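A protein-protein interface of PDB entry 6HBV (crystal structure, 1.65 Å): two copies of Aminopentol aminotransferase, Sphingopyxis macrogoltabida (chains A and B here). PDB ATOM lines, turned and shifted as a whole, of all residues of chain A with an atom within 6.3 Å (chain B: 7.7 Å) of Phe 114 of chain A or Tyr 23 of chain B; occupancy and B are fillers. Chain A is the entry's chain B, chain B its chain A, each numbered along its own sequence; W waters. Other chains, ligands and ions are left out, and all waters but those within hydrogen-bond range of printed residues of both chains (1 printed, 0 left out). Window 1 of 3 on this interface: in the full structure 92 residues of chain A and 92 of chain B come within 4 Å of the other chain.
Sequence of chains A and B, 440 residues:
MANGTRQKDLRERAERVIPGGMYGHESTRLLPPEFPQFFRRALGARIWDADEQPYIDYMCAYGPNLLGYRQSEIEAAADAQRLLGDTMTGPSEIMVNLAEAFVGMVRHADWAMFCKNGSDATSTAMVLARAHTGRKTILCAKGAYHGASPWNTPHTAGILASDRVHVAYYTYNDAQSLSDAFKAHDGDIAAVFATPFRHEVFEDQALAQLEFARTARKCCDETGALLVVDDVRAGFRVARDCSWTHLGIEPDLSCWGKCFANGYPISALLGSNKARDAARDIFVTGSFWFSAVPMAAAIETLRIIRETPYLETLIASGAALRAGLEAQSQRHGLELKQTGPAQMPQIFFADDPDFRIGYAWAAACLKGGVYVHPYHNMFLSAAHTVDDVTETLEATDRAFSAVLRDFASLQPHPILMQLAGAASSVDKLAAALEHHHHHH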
ATOM      1  N   MET A  95     -26.881 -19.057  38.016  1.00  0.00           N
ATOM      2  CA  MET A  95     -27.084 -19.099  36.570  1.00  0.00           C
ATOM      3  C   MET A  95     -25.844 -19.666  35.887  1.00  0.00           C
ATOM      4  O   MET A  95     -25.944 -20.415  34.879  1.00  0.00           O
ATOM      5  CB  MET A  95     -27.433 -17.717  36.030  1.00  0.00           C
ATOM      6  CG  MET A  95     -27.772 -17.705  34.584  1.00  0.00           C
ATOM      7  SD  MET A  95     -28.102 -16.039  33.995  1.00  0.00           S
ATOM      8  CE  MET A  95     -28.490 -16.408  32.286  1.00  0.00           C
ATOM      9  N   LEU A  98     -25.748 -23.374  36.383  1.00  0.00           N
ATOM     10  CA  LEU A  98     -26.751 -24.043  35.551  1.00  0.00           C
ATOM     11  C   LEU A  98     -26.235 -24.145  34.118  1.00  0.00           C
ATOM     12  O   LEU A  98     -26.316 -25.227  33.494  1.00  0.00           O
ATOM     13  CB  LEU A  98     -28.087 -23.280  35.575  1.00  0.00           C
ATOM     14  CG  LEU A  98     -29.133 -23.809  34.603  1.00  0.00           C
ATOM     15  CD1 LEU A  98     -29.347 -25.317  34.805  1.00  0.00           C
ATOM     16  CD2 LEU A  98     -30.449 -23.031  34.753  1.00  0.00           C
ATOM     17  N   ALA A  99     -25.705 -23.035  33.594  1.00  0.00           N
ATOM     18  CA  ALA A  99     -25.170 -23.045  32.248  1.00  0.00           C
ATOM     19  C   ALA A  99     -24.034 -24.080  32.125  1.00  0.00           C
ATOM     20  O   ALA A  99     -23.994 -24.855  31.157  1.00  0.00           O
ATOM     21  CB  ALA A  99     -24.743 -21.665  31.827  1.00  0.00           C
ATOM     22  N   PHE A 102     -25.581 -27.639  32.121  1.00  0.00           N
ATOM     23  CA  PHE A 102     -26.398 -27.980  30.935  1.00  0.00           C
ATOM     24  C   PHE A 102     -25.448 -28.159  29.760  1.00  0.00           C
ATOM     25  O   PHE A 102     -25.585 -29.150  29.007  1.00  0.00           O
ATOM     26  CB  PHE A 102     -27.517 -26.948  30.701  1.00  0.00           C
ATOM     27  CG  PHE A 102     -28.793 -27.493  30.099  1.00  0.00           C
ATOM     28  CD1 PHE A 102     -28.778 -28.480  29.128  1.00  0.00           C
ATOM     29  CD2 PHE A 102     -30.023 -27.007  30.506  1.00  0.00           C
ATOM     30  CE1 PHE A 102     -29.960 -28.964  28.594  1.00  0.00           C
ATOM     31  CE2 PHE A 102     -31.200 -27.487  29.967  1.00  0.00           C
ATOM     32  CZ  PHE A 102     -31.173 -28.467  29.009  1.00  0.00           C
ATOM     33  N   ALA A 112     -25.360 -21.820  26.730  1.00  0.00           N
ATOM     34  CA  ALA A 112     -26.784 -21.909  26.997  1.00  0.00           C
ATOM     35  C   ALA A 112     -27.346 -20.504  27.205  1.00  0.00           C
ATOM     36  O   ALA A 112     -26.662 -19.611  27.698  1.00  0.00           O
ATOM     37  CB  ALA A 112     -27.038 -22.813  28.187  1.00  0.00           C
ATOM     38  N   MET A 113     -28.616 -20.328  26.819  1.00  0.00           N
ATOM     39  CA  MET A 113     -29.426 -19.218  27.190  1.00  0.00           C
ATOM     40  C   MET A 113     -30.725 -19.747  27.821  1.00  0.00           C
ATOM     41  O   MET A 113     -31.267 -20.759  27.376  1.00  0.00           O
ATOM     42  CB  MET A 113     -29.731 -18.370  25.957  1.00  0.00           C
ATOM     43  CG  MET A 113     -28.476 -17.763  25.305  1.00  0.00           C
ATOM     44  SD  MET A 113     -28.817 -16.915  23.725  1.00  0.00           S
ATOM     45  CE  MET A 113     -29.498 -15.378  24.309  1.00  0.00           C
ATOM     46  N   PHE A 114     -31.212 -19.060  28.854  1.00  0.00           N
ATOM     47  CA  PHE A 114     -32.412 -19.448  29.570  1.00  0.00           C
ATOM     48  C   PHE A 114     -33.541 -18.446  29.352  1.00  0.00           C
ATOM     49  O   PHE A 114     -33.330 -17.236  29.228  1.00  0.00           O
ATOM     50  CB  PHE A 114     -32.083 -19.637  31.058  1.00  0.00           C
ATOM     51  CG  PHE A 114     -31.033 -20.710  31.183  1.00  0.00           C
ATOM     52  CD1 PHE A 114     -31.368 -22.037  30.948  1.00  0.00           C
ATOM     53  CD2 PHE A 114     -29.729 -20.398  31.519  1.00  0.00           C
ATOM     54  CE1 PHE A 114     -30.411 -23.036  31.051  1.00  0.00           C
ATOM     55  CE2 PHE A 114     -28.767 -21.398  31.628  1.00  0.00           C
ATOM     56  CZ  PHE A 114     -29.109 -22.700  31.391  1.00  0.00           C
ATOM     57  N   CYS A 115     -34.751 -18.990  29.319  1.00  0.00           N
ATOM     58  CA  CYS A 115     -35.980 -18.232  29.071  1.00  0.00           C
ATOM     59  C   CYS A 115     -37.113 -18.914  29.855  1.00  0.00           C
ATOM     60  O   CYS A 115     -36.815 -19.691  30.769  1.00  0.00           O
ATOM     61  CB  CYS A 115     -36.153 -18.073  27.570  1.00  0.00           C
ATOM     62  SG  CYS A 115     -36.167 -19.644  26.656  1.00  0.00           S
ATOM     63  N   LYS A 116     -38.386 -18.637  29.525  1.00  0.00           N
ATOM     64  CA  LYS A 116     -39.508 -19.162  30.246  1.00  0.00           C
ATOM     65  C   LYS A 116     -40.193 -20.288  29.474  1.00  0.00           C
ATOM     66  O   LYS A 116     -40.237 -21.471  29.908  1.00  0.00           O
ATOM     67  CB  LYS A 116     -40.503 -18.057  30.610  1.00  0.00           C
ATOM     68  CG  LYS A 116     -40.071 -17.212  31.803  1.00  0.00           C
ATOM     69  CD  LYS A 116     -39.915 -17.976  33.104  1.00  0.00           C
ATOM     70  CE  LYS A 116     -38.467 -18.109  33.521  1.00  0.00           C
ATOM     71  NZ  LYS A 116     -38.380 -18.584  34.912  1.00  0.00           N
ATOM     72  N   PHE A 260     -37.074 -30.023  32.440  1.00  0.00           N
ATOM     73  CA  PHE A 260     -35.684 -30.095  32.922  1.00  0.00           C
ATOM     74  C   PHE A 260     -35.557 -29.400  34.290  1.00  0.00           C
ATOM     75  O   PHE A 260     -34.483 -29.419  34.835  1.00  0.00           O
ATOM     76  CB  PHE A 260     -34.609 -29.661  31.919  1.00  0.00           C
ATOM     77  CG  PHE A 260     -34.525 -28.204  31.570  1.00  0.00           C
ATOM     78  CD1 PHE A 260     -33.975 -27.296  32.440  1.00  0.00           C
ATOM     79  CD2 PHE A 260     -35.005 -27.753  30.343  1.00  0.00           C
ATOM     80  CE1 PHE A 260     -33.903 -25.949  32.110  1.00  0.00           C
ATOM     81  CE2 PHE A 260     -34.931 -26.415  30.004  1.00  0.00           C
ATOM     82  CZ  PHE A 260     -34.381 -25.514  30.893  1.00  0.00           C
ATOM     83  N   ILE A 266     -38.996 -22.988  33.152  1.00  0.00           N
ATOM     84  CA  ILE A 266     -37.721 -22.560  32.579  1.00  0.00           C
ATOM     85  C   ILE A 266     -37.534 -23.353  31.270  1.00  0.00           C
ATOM     86  O   ILE A 266     -37.921 -24.521  31.189  1.00  0.00           O
ATOM     87  CB  ILE A 266     -36.549 -22.739  33.587  1.00  0.00           C
ATOM     88  CG1 ILE A 266     -35.222 -22.344  32.943  1.00  0.00           C
ATOM     89  CG2 ILE A 266     -36.477 -24.153  34.125  1.00  0.00           C
ATOM     90  CD1 ILE A 266     -34.084 -22.112  33.923  1.00  0.00           C
ATOM     91  N   SER A 267     -36.943 -22.684  30.261  1.00  0.00           N
ATOM     92  CA  SER A 267     -36.676 -23.239  28.964  1.00  0.00           C
ATOM     93  C   SER A 267     -35.256 -22.786  28.587  1.00  0.00           C
ATOM     94  O   SER A 267     -34.686 -21.902  29.235  1.00  0.00           O
ATOM     95  CB  SER A 267     -37.781 -22.833  27.967  1.00  0.00           C
ATOM     96  OG  SER A 267     -39.023 -23.390  28.388  1.00  0.00           O
ATOM     97  N   ALA A 268     -34.682 -23.391  27.549  1.00  0.00           N
ATOM     98  CA  ALA A 268     -33.306 -23.115  27.198  1.00  0.00           C
ATOM     99  C   ALA A 268     -33.062 -23.296  25.709  1.00  0.00           C
ATOM    100  O   ALA A 268     -33.683 -24.153  25.036  1.00  0.00           O
ATOM    101  CB  ALA A 268     -32.376 -24.039  27.951  1.00  0.00           C
ATOM    102  N   LEU A 269     -32.137 -22.473  25.224  1.00  0.00           N
ATOM    103  CA  LEU A 269     -31.474 -22.687  23.965  1.00  0.00           C
ATOM    104  C   LEU A 269     -30.009 -23.041  24.227  1.00  0.00           C
ATOM    105  O   LEU A 269     -29.271 -22.290  24.903  1.00  0.00           O
ATOM    106  CB  LEU A 269     -31.549 -21.414  23.135  1.00  0.00           C
ATOM    107  CG  LEU A 269     -30.918 -21.495  21.745  1.00  0.00           C
ATOM    108  CD1 LEU A 269     -31.601 -22.562  20.879  1.00  0.00           C
ATOM    109  CD2 LEU A 269     -31.004 -20.154  21.064  1.00  0.00           C
ATOM    110  N   LEU A 270     -29.601 -24.182  23.685  1.00  0.00           N
ATOM    111  CA  LEU A 270     -28.251 -24.710  23.784  1.00  0.00           C
ATOM    112  C   LEU A 270     -27.628 -24.586  22.408  1.00  0.00           C
ATOM    113  O   LEU A 270     -28.274 -24.926  21.426  1.00  0.00           O
ATOM    114  CB  LEU A 270     -28.253 -26.171  24.226  1.00  0.00           C
ATOM    115  CG  LEU A 270     -28.324 -26.459  25.733  1.00  0.00           C
ATOM    116  CD1 LEU A 270     -26.984 -26.338  26.406  1.00  0.00           C
ATOM    117  CD2 LEU A 270     -29.352 -25.593  26.444  1.00  0.00           C
ATOM    118  N   ALA A 279     -25.702 -15.266  18.687  1.00  0.00           N
ATOM    119  CA  ALA A 279     -26.437 -15.262  19.973  1.00  0.00           C
ATOM    120  C   ALA A 279     -26.205 -13.952  20.731  1.00  0.00           C
ATOM    121  O   ALA A 279     -27.130 -13.490  21.424  1.00  0.00           O
ATOM    122  CB  ALA A 279     -26.059 -16.443  20.831  1.00  0.00           C
ATOM    123  N   ILE A 282     -28.338 -10.771  18.745  1.00  0.00           N
ATOM    124  CA  ILE A 282     -29.792 -10.635  18.836  1.00  0.00           C
ATOM    125  C   ILE A 282     -30.165 -10.068  20.206  1.00  0.00           C
ATOM    126  O   ILE A 282     -29.365 -10.178  21.150  1.00  0.00           O
ATOM    127  CB  ILE A 282     -30.452 -11.988  18.604  1.00  0.00           C
ATOM    128  CG1 ILE A 282     -30.094 -12.986  19.715  1.00  0.00           C
ATOM    129  CG2 ILE A 282     -30.084 -12.501  17.226  1.00  0.00           C
ATOM    130  CD1 ILE A 282     -30.630 -14.379  19.511  1.00  0.00           C
ATOM    131  N   PHE A 283     -31.366  -9.477  20.290  1.00  0.00           N
ATOM    132  CA  PHE A 283     -31.891  -9.013  21.561  1.00  0.00           C
ATOM    133  C   PHE A 283     -33.138  -9.806  21.920  1.00  0.00           C
ATOM    134  O   PHE A 283     -34.215  -9.615  21.358  1.00  0.00           O
ATOM    135  CB  PHE A 283     -32.186  -7.520  21.579  1.00  0.00           C
ATOM    136  CG  PHE A 283     -32.595  -7.051  22.951  1.00  0.00           C
ATOM    137  CD1 PHE A 283     -31.628  -6.814  23.925  1.00  0.00           C
ATOM    138  CD2 PHE A 283     -33.923  -6.853  23.267  1.00  0.00           C
ATOM    139  CE1 PHE A 283     -31.986  -6.377  25.196  1.00  0.00           C
ATOM    140  CE2 PHE A 283     -34.287  -6.419  24.540  1.00  0.00           C
ATOM    141  CZ  PHE A 283     -33.319  -6.183  25.500  1.00  0.00           C
ATOM    142  N   VAL A 284     -32.929 -10.697  22.888  1.00  0.00           N
ATOM    143  CA  VAL A 284     -33.985 -11.467  23.536  1.00  0.00           C
ATOM    144  C   VAL A 284     -33.893 -11.304  25.065  1.00  0.00           C
ATOM    145  O   VAL A 284     -32.817 -11.285  25.629  1.00  0.00           O
ATOM    146  CB  VAL A 284     -33.897 -12.934  23.103  1.00  0.00           C
ATOM    147  CG1 VAL A 284     -34.189 -13.068  21.609  1.00  0.00           C
ATOM    148  CG2 VAL A 284     -32.544 -13.556  23.445  1.00  0.00           C
ATOM    149  N   THR A 285     -35.054 -11.191  25.716  1.00  0.00           N
ATOM    150  CA  THR A 285     -35.085 -11.032  27.139  1.00  0.00           C
ATOM    151  C   THR A 285     -36.506 -11.239  27.662  1.00  0.00           C
ATOM    152  O   THR A 285     -37.481 -11.232  26.911  1.00  0.00           O
ATOM    153  CB  THR A 285     -34.537  -9.663  27.550  1.00  0.00           C
ATOM    154  OG1 THR A 285     -34.135  -9.702  28.916  1.00  0.00           O
ATOM    155  CG2 THR A 285     -35.527  -8.538  27.345  1.00  0.00           C
ATOM    156  N   TRP A 289     -36.860 -14.166  33.054  1.00  0.00           N
ATOM    157  CA  TRP A 289     -35.878 -15.123  32.455  1.00  0.00           C
ATOM    158  C   TRP A 289     -34.637 -15.340  33.347  1.00  0.00           C
ATOM    159  O   TRP A 289     -33.893 -16.308  33.104  1.00  0.00           O
ATOM    160  CB  TRP A 289     -35.439 -14.629  31.067  1.00  0.00           C
ATOM    161  CG  TRP A 289     -36.498 -14.697  30.013  1.00  0.00           C
ATOM    162  CD1 TRP A 289     -37.858 -14.766  30.192  1.00  0.00           C
ATOM    163  CD2 TRP A 289     -36.274 -14.703  28.598  1.00  0.00           C
ATOM    164  NE1 TRP A 289     -38.478 -14.813  28.977  1.00  0.00           N
ATOM    165  CE2 TRP A 289     -37.542 -14.780  27.984  1.00  0.00           C
ATOM    166  CE3 TRP A 289     -35.133 -14.657  27.806  1.00  0.00           C
ATOM    167  CZ2 TRP A 289     -37.693 -14.806  26.602  1.00  0.00           C
ATOM    168  CZ3 TRP A 289     -35.279 -14.683  26.429  1.00  0.00           C
ATOM    169  CH2 TRP A 289     -36.546 -14.758  25.851  1.00  0.00           C
ATOM    170  N   PHE A 290     -34.412 -14.472  34.355  1.00  0.00           N
ATOM    171  CA  PHE A 290     -33.198 -14.521  35.158  1.00  0.00           C
ATOM    172  C   PHE A 290     -33.516 -14.966  36.589  1.00  0.00           C
ATOM    173  O   PHE A 290     -32.633 -14.884  37.431  1.00  0.00           O
ATOM    174  CB  PHE A 290     -32.437 -13.180  35.099  1.00  0.00           C
ATOM    175  CG  PHE A 290     -32.249 -12.749  33.668  1.00  0.00           C
ATOM    176  CD1 PHE A 290     -31.244 -13.296  32.894  1.00  0.00           C
ATOM    177  CD2 PHE A 290     -33.092 -11.806  33.100  1.00  0.00           C
ATOM    178  CE1 PHE A 290     -31.088 -12.899  31.575  1.00  0.00           C
ATOM    179  CE2 PHE A 290     -32.933 -11.409  31.782  1.00  0.00           C
ATOM    180  CZ  PHE A 290     -31.932 -11.958  31.029  1.00  0.00           C
ATOM    181  N   MET A 295     -34.004 -21.971  38.264  1.00  0.00           N
ATOM    182  CA  MET A 295     -32.636 -22.418  37.934  1.00  0.00           C
ATOM    183  C   MET A 295     -32.110 -23.420  38.979  1.00  0.00           C
ATOM    184  O   MET A 295     -31.422 -24.416  38.626  1.00  0.00           O
ATOM    185  CB  MET A 295     -31.693 -21.234  37.801  1.00  0.00           C
ATOM    186  CG  MET A 295     -32.066 -20.333  36.624  1.00  0.00           C
ATOM    187  SD  MET A 295     -30.776 -19.117  36.365  1.00  0.00           S
ATOM    188  CE  MET A 295     -31.555 -18.112  35.099  1.00  0.00           C
ATOM    189  N   VAL B  17     -19.758 -20.033  28.973  1.00  0.00           N
ATOM    190  CA  VAL B  17     -20.952 -20.942  28.788  1.00  0.00           C
ATOM    191  C   VAL B  17     -22.261 -20.183  28.505  1.00  0.00           C
ATOM    192  O   VAL B  17     -23.284 -20.811  28.334  1.00  0.00           O
ATOM    193  CB  VAL B  17     -21.106 -21.874  29.998  1.00  0.00           C
ATOM    194  CG1 VAL B  17     -19.962 -22.879  30.029  1.00  0.00           C
ATOM    195  CG2 VAL B  17     -21.179 -21.067  31.275  1.00  0.00           C
ATOM    196  N   ILE B  18     -22.198 -18.858  28.461  1.00  0.00           N
ATOM    197  CA  ILE B  18     -23.334 -17.989  28.196  1.00  0.00           C
ATOM    198  C   ILE B  18     -22.820 -16.982  27.179  1.00  0.00           C
ATOM    199  O   ILE B  18     -21.775 -16.381  27.387  1.00  0.00           O
ATOM    200  CB  ILE B  18     -23.883 -17.293  29.464  1.00  0.00           C
ATOM    201  CG1 ILE B  18     -24.283 -18.296  30.546  1.00  0.00           C
ATOM    202  CG2 ILE B  18     -25.037 -16.355  29.115  1.00  0.00           C
ATOM    203  CD1 ILE B  18     -24.631 -17.666  31.854  1.00  0.00           C
ATOM    204  N   PRO B  19     -23.519 -16.754  26.055  1.00  0.00           N
ATOM    205  CA  PRO B  19     -23.024 -15.842  25.030  1.00  0.00           C
ATOM    206  C   PRO B  19     -22.832 -14.453  25.660  1.00  0.00           C
ATOM    207  O   PRO B  19     -23.762 -13.849  26.151  1.00  0.00           O
ATOM    208  CB  PRO B  19     -24.140 -15.815  23.977  1.00  0.00           C
ATOM    209  CG  PRO B  19     -24.879 -17.108  24.196  1.00  0.00           C
ATOM    210  CD  PRO B  19     -24.813 -17.342  25.692  1.00  0.00           C
ATOM    211  N   GLY B  20     -21.587 -13.969  25.628  1.00  0.00           N
ATOM    212  CA  GLY B  20     -21.292 -12.657  26.159  1.00  0.00           C
ATOM    213  C   GLY B  20     -21.257 -12.622  27.681  1.00  0.00           C
ATOM    214  O   GLY B  20     -21.079 -11.546  28.206  1.00  0.00           O
ATOM    215  N   GLY B  21     -21.422 -13.764  28.374  1.00  0.00           N
ATOM    216  CA  GLY B  21     -21.481 -13.834  29.842  1.00  0.00           C
ATOM    217  C   GLY B  21     -22.851 -13.547  30.434  1.00  0.00           C
ATOM    218  O   GLY B  21     -23.109 -13.922  31.572  1.00  0.00           O
ATOM    219  N   MET B  22     -23.722 -12.885  29.662  1.00  0.00           N
ATOM    220  CA  MET B  22     -25.088 -12.535  30.024  1.00  0.00           C
ATOM    221  C   MET B  22     -25.732 -11.796  28.835  1.00  0.00           C
ATOM    222  O   MET B  22     -25.069 -11.464  27.881  1.00  0.00           O
ATOM    223  CB  MET B  22     -25.152 -11.709  31.319  1.00  0.00           C
ATOM    224  CG  MET B  22     -25.815 -12.479  32.447  1.00  0.00           C
ATOM    225  SD  MET B  22     -27.609 -12.695  32.236  1.00  0.00           S
ATOM    226  CE  MET B  22     -28.174 -11.023  32.545  1.00  0.00           C
ATOM    227  N   TYR B  23     -27.044 -11.557  28.920  1.00  0.00           N
ATOM    228  CA  TYR B  23     -27.837 -11.094  27.760  1.00  0.00           C
ATOM    229  C   TYR B  23     -29.082 -10.427  28.334  1.00  0.00           C
ATOM    230  O   TYR B  23     -29.420 -10.589  29.525  1.00  0.00           O
ATOM    231  CB  TYR B  23     -28.183 -12.234  26.788  1.00  0.00           C
ATOM    232  CG  TYR B  23     -28.893 -13.344  27.517  1.00  0.00           C
ATOM    233  CD1 TYR B  23     -30.264 -13.347  27.679  1.00  0.00           C
ATOM    234  CD2 TYR B  23     -28.178 -14.398  28.064  1.00  0.00           C
ATOM    235  CE1 TYR B  23     -30.916 -14.363  28.363  1.00  0.00           C
ATOM    236  CE2 TYR B  23     -28.816 -15.421  28.747  1.00  0.00           C
ATOM    237  CZ  TYR B  23     -30.192 -15.410  28.902  1.00  0.00           C
ATOM    238  OH  TYR B  23     -30.794 -16.440  29.594  1.00  0.00           O
ATOM    239  N   GLY B  24     -29.761  -9.677  27.473  1.00  0.00           N
ATOM    240  CA  GLY B  24     -31.039  -9.150  27.768  1.00  0.00           C
ATOM    241  C   GLY B  24     -30.966  -7.968  28.705  1.00  0.00           C
ATOM    242  O   GLY B  24     -29.922  -7.348  28.851  1.00  0.00           O
ATOM    243  N   HIS B  25     -32.109  -7.660  29.341  1.00  0.00           N
ATOM    244  CA  HIS B  25     -32.332  -6.346  29.994  1.00  0.00           C
ATOM    245  C   HIS B  25     -31.534  -6.224  31.305  1.00  0.00           C
ATOM    246  O   HIS B  25     -31.270  -5.112  31.754  1.00  0.00           O
ATOM    247  CB  HIS B  25     -33.835  -6.059  30.235  1.00  0.00           C
ATOM    248  CG  HIS B  25     -34.499  -6.898  31.291  1.00  0.00           C
ATOM    249  ND1 HIS B  25     -34.881  -8.232  31.080  1.00  0.00           N
ATOM    250  CD2 HIS B  25     -34.864  -6.608  32.567  1.00  0.00           C
ATOM    251  CE1 HIS B  25     -35.439  -8.697  32.200  1.00  0.00           C
ATOM    252  NE2 HIS B  25     -35.444  -7.735  33.116  1.00  0.00           N
ATOM    253  N   GLU B  26     -31.161  -7.354  31.908  1.00  0.00           N
ATOM    254  CA  GLU B  26     -30.392  -7.360  33.151  1.00  0.00           C
ATOM    255  C   GLU B  26     -28.876  -7.480  32.934  1.00  0.00           C
ATOM    256  O   GLU B  26     -28.131  -7.525  33.925  1.00  0.00           O
ATOM    257  CB  GLU B  26     -30.871  -8.484  34.064  1.00  0.00           C
ATOM    258  CG  GLU B  26     -32.275  -8.232  34.526  1.00  0.00           C
ATOM    259  CD  GLU B  26     -32.805  -9.180  35.566  1.00  0.00           C
ATOM    260  OE1 GLU B  26     -32.016  -9.999  36.106  1.00  0.00           O
ATOM    261  OE2 GLU B  26     -34.002  -9.100  35.835  1.00  0.00           O
ATOM    262  N   SER B  27     -28.408  -7.535  31.683  1.00  0.00           N
ATOM    263  CA  SER B  27     -26.992  -7.495  31.401  1.00  0.00           C
ATOM    264  C   SER B  27     -26.430  -6.133  31.823  1.00  0.00           C
ATOM    265  O   SER B  27     -27.049  -5.114  31.628  1.00  0.00           O
ATOM    266  CB  SER B  27     -26.672  -7.787  29.923  1.00  0.00           C
ATOM    267  OG  SER B  27     -25.336  -7.400  29.616  1.00  0.00           O
ATOM    268  N   THR B  28     -25.235  -6.154  32.409  1.00  0.00           N
ATOM    269  CA  THR B  28     -24.530  -4.952  32.814  1.00  0.00           C
ATOM    270  C   THR B  28     -23.603  -4.426  31.711  1.00  0.00           C
ATOM    271  O   THR B  28     -22.813  -3.559  31.975  1.00  0.00           O
ATOM    272  CB  THR B  28     -23.743  -5.200  34.108  1.00  0.00           C
ATOM    273  OG1 THR B  28     -22.830  -6.268  33.886  1.00  0.00           O
ATOM    274  CG2 THR B  28     -24.676  -5.502  35.257  1.00  0.00           C
ATOM    275  N   ARG B  29     -23.700  -4.943  30.482  1.00  0.00           N
ATOM    276  CA  ARG B  29     -22.762  -4.604  29.436  1.00  0.00           C
ATOM    277  C   ARG B  29     -22.671  -3.075  29.198  1.00  0.00           C
ATOM    278  O   ARG B  29     -21.578  -2.571  28.934  1.00  0.00           O
ATOM    279  CB  ARG B  29     -23.169  -5.321  28.145  1.00  0.00           C
ATOM    280  CG  ARG B  29     -22.239  -5.066  26.974  1.00  0.00           C
ATOM    281  CD  ARG B  29     -22.500  -6.002  25.814  1.00  0.00           C
ATOM    282  NE  ARG B  29     -21.366  -5.943  24.895  1.00  0.00           N
ATOM    283  CZ  ARG B  29     -21.376  -5.388  23.684  1.00  0.00           C
ATOM    284  NH1 ARG B  29     -20.263  -5.366  22.970  1.00  0.00           N
ATOM    285  NH2 ARG B  29     -22.485  -4.861  23.189  1.00  0.00           N
ATOM    286  N   GLN B  37     -22.955  -8.061  38.189  1.00  0.00           N
ATOM    287  CA  GLN B  37     -23.853  -8.789  37.287  1.00  0.00           C
ATOM    288  C   GLN B  37     -24.645  -9.855  38.066  1.00  0.00           C
ATOM    289  O   GLN B  37     -25.850 -10.007  37.839  1.00  0.00           O
ATOM    290  CB  GLN B  37     -23.042  -9.413  36.142  1.00  0.00           C
ATOM    291  CG  GLN B  37     -23.881 -10.240  35.159  1.00  0.00           C
ATOM    292  CD  GLN B  37     -24.879  -9.393  34.418  1.00  0.00           C
ATOM    293  OE1 GLN B  37     -24.592  -8.940  33.298  1.00  0.00           O
ATOM    294  NE2 GLN B  37     -26.041  -9.170  35.029  1.00  0.00           N
HETATM  295  O   HOH W   1     -30.324 -10.605  24.390  1.00  0.00           O
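No position is printed for both chains.
Of the 20 pairs that touch across the chains among the printed residues, none has its exchanged pair printed and touching as well.
Phe 114 of chain A touches just one residue of chain B: Tyr 23.
Printed residues of chain A within 4 Å of Tyr 23 of chain B: Met 95, Met 113, Phe 114, Val 284 and Phe 290.
Printed residues of chain A within 4 Å of Pro 19 of chain B: Ala 112 (3.5 Å), Met 113 (3.7 Å) and Ala 279 (3.6 Å).
Printed residues of chain A within 4 Å of Ile 18 of chain B: Ala 99 (3.6 Å) and Ala 112 (3.7 Å).
Of the printed residues of chain B, Ala 112 of chain A touches Val 17 (2.8 Å), Ile 18 (3.7 Å) and Pro 19 (3.5 Å).
Of the printed residues of chain B, Phe 290 of chain A touches Met 22 (3.5 Å), Tyr 23 (3.2 Å), His 25 (3.7 Å) and Glu 26 (3.4 Å).
The nearest residue of chain B that does not touch Phe 114 of chain A is Ile 18 of chain B (5.6 Å).
The nearest printed residue of chain A that does not touch Ile 18 of chain B is Met 95 of chain A (4.1 Å).
Water W1 lies within hydrogen-bond range of O of Val 284 of chain A, N of Gly 24 of chain B and O of Ile 282 of chain A.
A ring nitrogen (NE2) of His 25 of chain B is in hydrogen-bond range of the side-chain carboxylate (OE2) of Glu 26 of chain B (3.4 Å).
The backbone carbonyl oxygen (O) of Glu 26 of chain B sits at hydrogen-bond distance from the side-chain amide nitrogen (NE2) of Gln 37 of chain B, 2.9 Å away.
The backbone NH (N) of Met 113 of chain A is in hydrogen-bond range of the backbone carbonyl oxygen (O) of Leu 269 of chain A, at 2.8 Å.
Tyr 23 of chain B touches Met 95 of chain A.
Ile 18 of chain B touches Ala 99 of chain A (CG1 to CB, 3.6 Å).
Ala 112 of chain A touches Ile 18 of chain B.
Ala 112 of chain A touches Pro 19 of chain B.
Met 113 of chain A touches Tyr 23 of chain B.
O of Val 284 of chain A touches CA of Gly 24 of chain B, 3.5 Å away.
OG1 of Thr 285 of chain A touches CA of Gly 24 of chain B, 3.3 Å away.
Met 22 of chain B touches Phe 290 of chain A.
His 25 of chain B touches Phe 290 of chain A.
CB of Phe 290 of chain A touches OE1 of Glu 26 of chain B, 3.4 Å away.
Printed residues of chain A that touch a printed residue of chain B: Met 95, Ala 99, Ala 112, Met 113, Phe 114, Ala 279, Phe 283, Val 284, Thr 285 and Phe 290.
Hydrophobic or aromatic side chains of chain A within 4 Å of the printed part of chain B: Met 95, Ala 99, Met 113, Phe 114, Ala 279, Phe 283 and Phe 290.
Along chain A the printed residues that touch a printed residue of chain B span positions 95 to 290.
The backbone carbonyl oxygen of Val 17 of chain B lies within hydrogen-bond range of the backbone NH of Ala 112 of chain A (2.8 Å).
OH of Tyr 23 of chain B is in hydrogen-bond range of O of Phe 114 of chain A (2.7 Å).
ND1 of His 25 of chain B lies within hydrogen-bond range of OG1 of Thr 285 of chain A (2.7 Å).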
